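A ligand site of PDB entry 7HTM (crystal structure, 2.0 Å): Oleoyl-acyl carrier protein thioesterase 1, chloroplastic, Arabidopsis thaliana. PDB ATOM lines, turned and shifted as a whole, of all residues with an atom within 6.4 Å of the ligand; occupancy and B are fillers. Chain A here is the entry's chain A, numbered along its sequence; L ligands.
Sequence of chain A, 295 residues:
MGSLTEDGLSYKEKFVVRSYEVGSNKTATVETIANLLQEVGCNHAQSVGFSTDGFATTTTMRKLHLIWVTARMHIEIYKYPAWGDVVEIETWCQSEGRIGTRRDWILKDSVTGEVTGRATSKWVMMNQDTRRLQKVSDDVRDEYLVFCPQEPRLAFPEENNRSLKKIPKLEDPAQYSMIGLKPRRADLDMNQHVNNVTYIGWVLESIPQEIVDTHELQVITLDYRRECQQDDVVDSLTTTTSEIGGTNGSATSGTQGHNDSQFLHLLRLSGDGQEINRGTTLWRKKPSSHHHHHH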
ATOM      1  N   LEU A   4      14.414 -17.131  17.587  1.00  0.00           N
ATOM      2  CA  LEU A   4      15.348 -18.135  17.078  1.00  0.00           C
ATOM      3  C   LEU A   4      16.761 -17.586  17.224  1.00  0.00           C
ATOM      4  O   LEU A   4      16.973 -16.373  17.148  1.00  0.00           O
ATOM      5  CB  LEU A   4      15.104 -18.383  15.579  1.00  0.00           C
ATOM      6  CG  LEU A   4      13.816 -19.059  15.178  1.00  0.00           C
ATOM      7  CD1 LEU A   4      13.504 -18.784  13.729  1.00  0.00           C
ATOM      8  CD2 LEU A   4      13.888 -20.547  15.395  1.00  0.00           C
ATOM      9  N   GLY A  41       8.465 -24.600  23.450  1.00  0.00           N
ATOM     10  CA  GLY A  41       8.361 -25.534  22.329  1.00  0.00           C
ATOM     11  C   GLY A  41       7.314 -25.059  21.322  1.00  0.00           C
ATOM     12  O   GLY A  41       7.517 -25.203  20.108  1.00  0.00           O
ATOM     13  N   HIS A  44       8.677 -21.967  19.443  1.00  0.00           N
ATOM     14  CA  HIS A  44       9.671 -22.402  18.470  1.00  0.00           C
ATOM     15  C   HIS A  44       8.941 -22.850  17.178  1.00  0.00           C
ATOM     16  O   HIS A  44       9.292 -22.386  16.106  1.00  0.00           O
ATOM     17  CB  HIS A  44      10.551 -23.519  19.057  1.00  0.00           C
ATOM     18  CG  HIS A  44      11.632 -24.011  18.138  1.00  0.00           C
ATOM     19  ND1 HIS A  44      12.289 -25.209  18.361  1.00  0.00           N
ATOM     20  CD2 HIS A  44      12.132 -23.458  17.007  1.00  0.00           C
ATOM     21  CE1 HIS A  44      13.167 -25.339  17.386  1.00  0.00           C
ATOM     22  NE2 HIS A  44      13.108 -24.319  16.543  1.00  0.00           N
ATOM     23  N   ALA A  45       7.920 -23.726  17.287  1.00  0.00           N
ATOM     24  CA  ALA A  45       7.145 -24.186  16.111  1.00  0.00           C
ATOM     25  C   ALA A  45       6.433 -23.035  15.371  1.00  0.00           C
ATOM     26  O   ALA A  45       6.514 -22.968  14.150  1.00  0.00           O
ATOM     27  CB  ALA A  45       6.161 -25.273  16.518  1.00  0.00           C
ATOM     28  N   GLN A  46       5.803 -22.096  16.089  1.00  0.00           N
ATOM     29  CA  GLN A  46       5.166 -20.941  15.469  1.00  0.00           C
ATOM     30  C   GLN A  46       6.160 -20.055  14.716  1.00  0.00           C
ATOM     31  O   GLN A  46       5.839 -19.572  13.627  1.00  0.00           O
ATOM     32  CB  GLN A  46       4.453 -20.066  16.523  1.00  0.00           C
ATOM     33  CG  GLN A  46       3.184 -20.662  17.121  1.00  0.00           C
ATOM     34  CD  GLN A  46       2.600 -19.753  18.189  1.00  0.00           C
ATOM     35  OE1 GLN A  46       2.699 -20.013  19.407  1.00  0.00           O
ATOM     36  NE2 GLN A  46       1.977 -18.663  17.762  1.00  0.00           N
ATOM     37  N   VAL A  48       8.725 -20.758  13.050  1.00  0.00           N
ATOM     38  CA  VAL A  48       9.214 -21.328  11.795  1.00  0.00           C
ATOM     39  C   VAL A  48       8.075 -21.836  10.891  1.00  0.00           C
ATOM     40  O   VAL A  48       8.324 -22.600   9.972  1.00  0.00           O
ATOM     41  CB  VAL A  48      10.318 -22.395  12.000  1.00  0.00           C
ATOM     42  CG1 VAL A  48      11.600 -21.765  12.546  1.00  0.00           C
ATOM     43  CG2 VAL A  48       9.839 -23.504  12.923  1.00  0.00           C
ATOM     44  N   PHE A  50       5.007 -23.545  11.768  1.00  0.00           N
ATOM     45  CA  PHE A  50       4.258 -24.754  12.111  1.00  0.00           C
ATOM     46  C   PHE A  50       3.068 -24.426  13.016  1.00  0.00           C
ATOM     47  O   PHE A  50       2.508 -23.328  12.926  1.00  0.00           O
ATOM     48  CB  PHE A  50       5.155 -25.803  12.780  1.00  0.00           C
ATOM     49  CG  PHE A  50       6.214 -26.411  11.900  1.00  0.00           C
ATOM     50  CD1 PHE A  50       5.966 -27.566  11.187  1.00  0.00           C
ATOM     51  CD2 PHE A  50       7.477 -25.850  11.828  1.00  0.00           C
ATOM     52  CE1 PHE A  50       6.962 -28.130  10.394  1.00  0.00           C
ATOM     53  CE2 PHE A  50       8.464 -26.424  11.041  1.00  0.00           C
ATOM     54  CZ  PHE A  50       8.190 -27.561  10.326  1.00  0.00           C
ATOM     55  N   ALA A  56       2.911 -29.345  16.084  1.00  0.00           N
ATOM     56  CA  ALA A  56       3.932 -29.008  15.094  1.00  0.00           C
ATOM     57  C   ALA A  56       3.716 -29.853  13.834  1.00  0.00           C
ATOM     58  O   ALA A  56       4.644 -30.488  13.329  1.00  0.00           O
ATOM     59  CB  ALA A  56       5.321 -29.244  15.670  1.00  0.00           C
ATOM     60  N   THR A  57       2.478 -29.874  13.333  1.00  0.00           N
ATOM     61  CA  THR A  57       2.143 -30.672  12.159  1.00  0.00           C
ATOM     62  C   THR A  57       2.595 -30.026  10.860  1.00  0.00           C
ATOM     63  O   THR A  57       2.298 -28.854  10.609  1.00  0.00           O
ATOM     64  CB  THR A  57       0.650 -30.977  12.150  1.00  0.00           C
ATOM     65  OG1 THR A  57      -0.065 -29.752  12.063  1.00  0.00           O
ATOM     66  CG2 THR A  57       0.206 -31.731  13.380  1.00  0.00           C
ATOM     67  N   THR A  58       3.309 -30.793  10.023  1.00  0.00           N
ATOM     68  CA  THR A  58       3.750 -30.330   8.705  1.00  0.00           C
ATOM     69  C   THR A  58       2.541 -30.293   7.737  1.00  0.00           C
ATOM     70  O   THR A  58       1.426 -30.646   8.122  1.00  0.00           O
ATOM     71  CB  THR A  58       4.948 -31.192   8.208  1.00  0.00           C
ATOM     72  OG1 THR A  58       4.466 -32.473   7.766  1.00  0.00           O
ATOM     73  CG2 THR A  58       6.047 -31.363   9.257  1.00  0.00           C
ATOM     74  N   MET A  61       1.434 -33.898   7.218  1.00  0.00           N
ATOM     75  CA  MET A  61       0.819 -34.464   8.414  1.00  0.00           C
ATOM     76  C   MET A  61      -0.637 -34.020   8.548  1.00  0.00           C
ATOM     77  O   MET A  61      -1.469 -34.816   8.984  1.00  0.00           O
ATOM     78  CB  MET A  61       1.609 -34.071   9.669  1.00  0.00           C
ATOM     79  CG  MET A  61       2.914 -34.810   9.800  1.00  0.00           C
ATOM     80  SD  MET A  61       3.938 -34.165  11.147  1.00  0.00           S
ATOM     81  CE  MET A  61       2.906 -34.527  12.542  1.00  0.00           C
ATOM     82  N   TRP A  68       2.116 -35.371  16.328  1.00  0.00           N
ATOM     83  CA  TRP A  68       3.250 -35.764  17.158  1.00  0.00           C
ATOM     84  C   TRP A  68       2.690 -35.935  18.558  1.00  0.00           C
ATOM     85  O   TRP A  68       2.006 -35.037  19.058  1.00  0.00           O
ATOM     86  CB  TRP A  68       4.332 -34.661  17.174  1.00  0.00           C
ATOM     87  CG  TRP A  68       5.119 -34.547  15.905  1.00  0.00           C
ATOM     88  CD1 TRP A  68       5.112 -33.500  15.023  1.00  0.00           C
ATOM     89  CD2 TRP A  68       6.047 -35.517  15.379  1.00  0.00           C
ATOM     90  NE1 TRP A  68       5.968 -33.771  13.983  1.00  0.00           N
ATOM     91  CE2 TRP A  68       6.568 -34.986  14.182  1.00  0.00           C
ATOM     92  CE3 TRP A  68       6.505 -36.764  15.815  1.00  0.00           C
ATOM     93  CZ2 TRP A  68       7.499 -35.672  13.412  1.00  0.00           C
ATOM     94  CZ3 TRP A  68       7.437 -37.437  15.052  1.00  0.00           C
ATOM     95  CH2 TRP A  68       7.900 -36.908  13.862  1.00  0.00           C
ATOM     96  N   TRP A  92      15.481 -27.006  21.109  1.00  0.00           N
ATOM     97  CA  TRP A  92      15.748 -27.417  19.744  1.00  0.00           C
ATOM     98  C   TRP A  92      15.176 -28.831  19.511  1.00  0.00           C
ATOM     99  O   TRP A  92      14.862 -29.537  20.478  1.00  0.00           O
ATOM    100  CB  TRP A  92      17.268 -27.371  19.411  1.00  0.00           C
ATOM    101  CG  TRP A  92      18.079 -28.429  20.104  1.00  0.00           C
ATOM    102  CD1 TRP A  92      18.439 -29.644  19.609  1.00  0.00           C
ATOM    103  CD2 TRP A  92      18.672 -28.337  21.414  1.00  0.00           C
ATOM    104  NE1 TRP A  92      19.154 -30.351  20.554  1.00  0.00           N
ATOM    105  CE2 TRP A  92      19.342 -29.547  21.655  1.00  0.00           C
ATOM    106  CE3 TRP A  92      18.729 -27.319  22.384  1.00  0.00           C
ATOM    107  CZ2 TRP A  92      20.081 -29.779  22.821  1.00  0.00           C
ATOM    108  CZ3 TRP A  92      19.388 -27.579  23.565  1.00  0.00           C
ATOM    109  CH2 TRP A  92      20.073 -28.788  23.773  1.00  0.00           C
ATOM    110  N   CYS A  93      15.024 -29.220  18.248  1.00  0.00           N
ATOM    111  CA  CYS A  93      14.531 -30.542  17.898  1.00  0.00           C
ATOM    112  C   CYS A  93      15.577 -31.315  17.087  1.00  0.00           C
ATOM    113  O   CYS A  93      16.395 -30.717  16.408  1.00  0.00           O
ATOM    114  CB  CYS A  93      13.213 -30.461  17.140  1.00  0.00           C
ATOM    115  SG  CYS A  93      11.911 -29.565  18.003  1.00  0.00           S
ATOM    116  N   GLN A  94      15.507 -32.645  17.142  1.00  0.00           N
ATOM    117  CA  GLN A  94      16.386 -33.480  16.357  1.00  0.00           C
ATOM    118  C   GLN A  94      15.613 -34.685  15.861  1.00  0.00           C
ATOM    119  O   GLN A  94      14.783 -35.245  16.559  1.00  0.00           O
ATOM    120  CB  GLN A  94      17.639 -33.917  17.125  1.00  0.00           C
ATOM    121  CG  GLN A  94      18.747 -32.861  17.105  1.00  0.00           C
ATOM    122  CD  GLN A  94      20.082 -33.475  16.851  1.00  0.00           C
ATOM    123  OE1 GLN A  94      20.467 -34.447  17.498  1.00  0.00           O
ATOM    124  NE2 GLN A  94      20.826 -32.908  15.924  1.00  0.00           N
ATOM    125  N   THR A 101      10.823 -38.135  16.639  1.00  0.00           N
ATOM    126  CA  THR A 101      11.575 -36.915  16.870  1.00  0.00           C
ATOM    127  C   THR A 101      11.926 -36.766  18.367  1.00  0.00           C
ATOM    128  O   THR A 101      11.422 -37.499  19.207  1.00  0.00           O
ATOM    129  CB  THR A 101      10.829 -35.670  16.303  1.00  0.00           C
ATOM    130  OG1 THR A 101       9.518 -35.596  16.826  1.00  0.00           O
ATOM    131  CG2 THR A 101      10.889 -35.588  14.817  1.00  0.00           C
ATOM    132  N   ARG A 103      12.793 -33.521  21.349  1.00  0.00           N
ATOM    133  CA  ARG A 103      12.897 -32.099  21.641  1.00  0.00           C
ATOM    134  C   ARG A 103      13.718 -31.998  22.911  1.00  0.00           C
ATOM    135  O   ARG A 103      13.432 -32.719  23.872  1.00  0.00           O
ATOM    136  CB  ARG A 103      11.538 -31.363  21.744  1.00  0.00           C
ATOM    137  CG  ARG A 103      11.724 -29.917  22.223  1.00  0.00           C
ATOM    138  CD  ARG A 103      10.497 -29.045  22.168  1.00  0.00           C
ATOM    139  NE  ARG A 103      10.013 -28.765  20.814  1.00  0.00           N
ATOM    140  CZ  ARG A 103      10.474 -27.802  20.027  1.00  0.00           C
ATOM    141  NH1 ARG A 103       9.925 -27.590  18.837  1.00  0.00           N
ATOM    142  NH2 ARG A 103      11.505 -27.047  20.410  1.00  0.00           N
ATOM    143  N   TYR A 144      10.836 -31.049   8.000  1.00  0.00           N
ATOM    144  CA  TYR A 144      11.245 -30.504   9.293  1.00  0.00           C
ATOM    145  C   TYR A 144      12.776 -30.535   9.521  1.00  0.00           C
ATOM    146  O   TYR A 144      13.248 -29.818  10.398  1.00  0.00           O
ATOM    147  CB  TYR A 144      10.491 -31.156  10.469  1.00  0.00           C
ATOM    148  CG  TYR A 144      10.848 -32.596  10.750  1.00  0.00           C
ATOM    149  CD1 TYR A 144      12.002 -32.923  11.457  1.00  0.00           C
ATOM    150  CD2 TYR A 144       9.975 -33.632  10.441  1.00  0.00           C
ATOM    151  CE1 TYR A 144      12.332 -34.240  11.735  1.00  0.00           C
ATOM    152  CE2 TYR A 144      10.283 -34.945  10.730  1.00  0.00           C
ATOM    153  CZ  TYR A 144      11.475 -35.260  11.367  1.00  0.00           C
ATOM    154  OH  TYR A 144      11.791 -36.568  11.660  1.00  0.00           O
ATOM    155  N   PHE A 147      15.036 -27.388   9.824  1.00  0.00           N
ATOM    156  CA  PHE A 147      14.864 -26.634  11.082  1.00  0.00           C
ATOM    157  C   PHE A 147      15.590 -27.282  12.275  1.00  0.00           C
ATOM    158  O   PHE A 147      15.460 -26.815  13.405  1.00  0.00           O
ATOM    159  CB  PHE A 147      13.363 -26.495  11.414  1.00  0.00           C
ATOM    160  CG  PHE A 147      12.561 -25.906  10.276  1.00  0.00           C
ATOM    161  CD1 PHE A 147      12.701 -24.576   9.930  1.00  0.00           C
ATOM    162  CD2 PHE A 147      11.720 -26.699   9.531  1.00  0.00           C
ATOM    163  CE1 PHE A 147      12.000 -24.049   8.855  1.00  0.00           C
ATOM    164  CE2 PHE A 147      11.012 -26.166   8.459  1.00  0.00           C
ATOM    165  CZ  PHE A 147      11.165 -24.847   8.130  1.00  0.00           C
ATOM    166  N   CYS A 148      16.357 -28.358  12.036  1.00  0.00           N
ATOM    167  CA  CYS A 148      17.060 -29.113  13.057  1.00  0.00           C
ATOM    168  C   CYS A 148      18.557 -29.051  12.833  1.00  0.00           C
ATOM    169  O   CYS A 148      19.006 -29.081  11.683  1.00  0.00           O
ATOM    170  CB  CYS A 148      16.573 -30.553  13.030  1.00  0.00           C
ATOM    171  SG  CYS A 148      14.803 -30.759  13.354  1.00  0.00           S
HETATM  172  C1  LIG L   1       8.220 -30.003  13.539  1.00  0.00           C
HETATM  173  C2  LIG L   1      11.453 -26.304  14.341  1.00  0.00           C
HETATM  174  S1  LIG L   1      10.223 -27.399  14.935  1.00  0.00           S
HETATM  175  O1  LIG L   1       8.930 -26.890  14.590  1.00  0.00           O
HETATM  176  O2  LIG L   1      10.517 -27.645  16.319  1.00  0.00           O
HETATM  177  N1  LIG L   1      10.435 -28.823  14.126  1.00  0.00           N
HETATM  178  C3  LIG L   1       9.537 -29.964  14.327  1.00  0.00           C
HETATM  179  C4  LIG L   1      10.119 -31.357  14.203  1.00  0.00           C
HETATM  180  C5  LIG L   1       8.867 -32.217  14.228  1.00  0.00           C
HETATM  181  C6  LIG L   1       7.927 -31.480  13.310  1.00  0.00           C
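NH1 of Arg 103 sits at hydrogen-bond distance from O2 of the ligand (2.6 Å). SG of Cys 93 lies within hydrogen-bond range of O2 of the ligand (2.9 Å).
The guanidinium group of Arg 103 sits at hydrogen-bond distance from the side-chain sulfur of Cys 93. NH2 of Arg 103 lies within hydrogen-bond range of ND1 of His 44, 2.9 Å away. O of Cys 93 sits close to SG of Cys 148, at 3.4 Å. The indole nitrogen of Trp 68 lies close to the side-chain sulfur of Met 61, at 3.5 Å. The backbone carbonyl oxygen (O) of Ala 45 is in hydrogen-bond range of the backbone NH (N) of Phe 50, 2.9 Å away. The backbone carbonyl oxygen of Tyr 144 is in hydrogen-bond range of the side-chain sulfur of Cys 148 (3.5 Å).
Residues that only touch the ligand: Trp 68 (3.1 Å), Phe 50 (3.3 Å), His 44 (3.4 Å), Ala 56 (3.4 Å), Phe 147 (3.5 Å), Val 48 (3.5 Å), Ala 45 (3.6 Å), Tyr 144 (3.7 Å) and Thr 101 (3.97 Å). Hydrophobic or aromatic side chains that line the ligand: His 44, Ala 45, Val 48, Phe 50, Ala 56, Trp 68, Tyr 144 and Phe 147.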
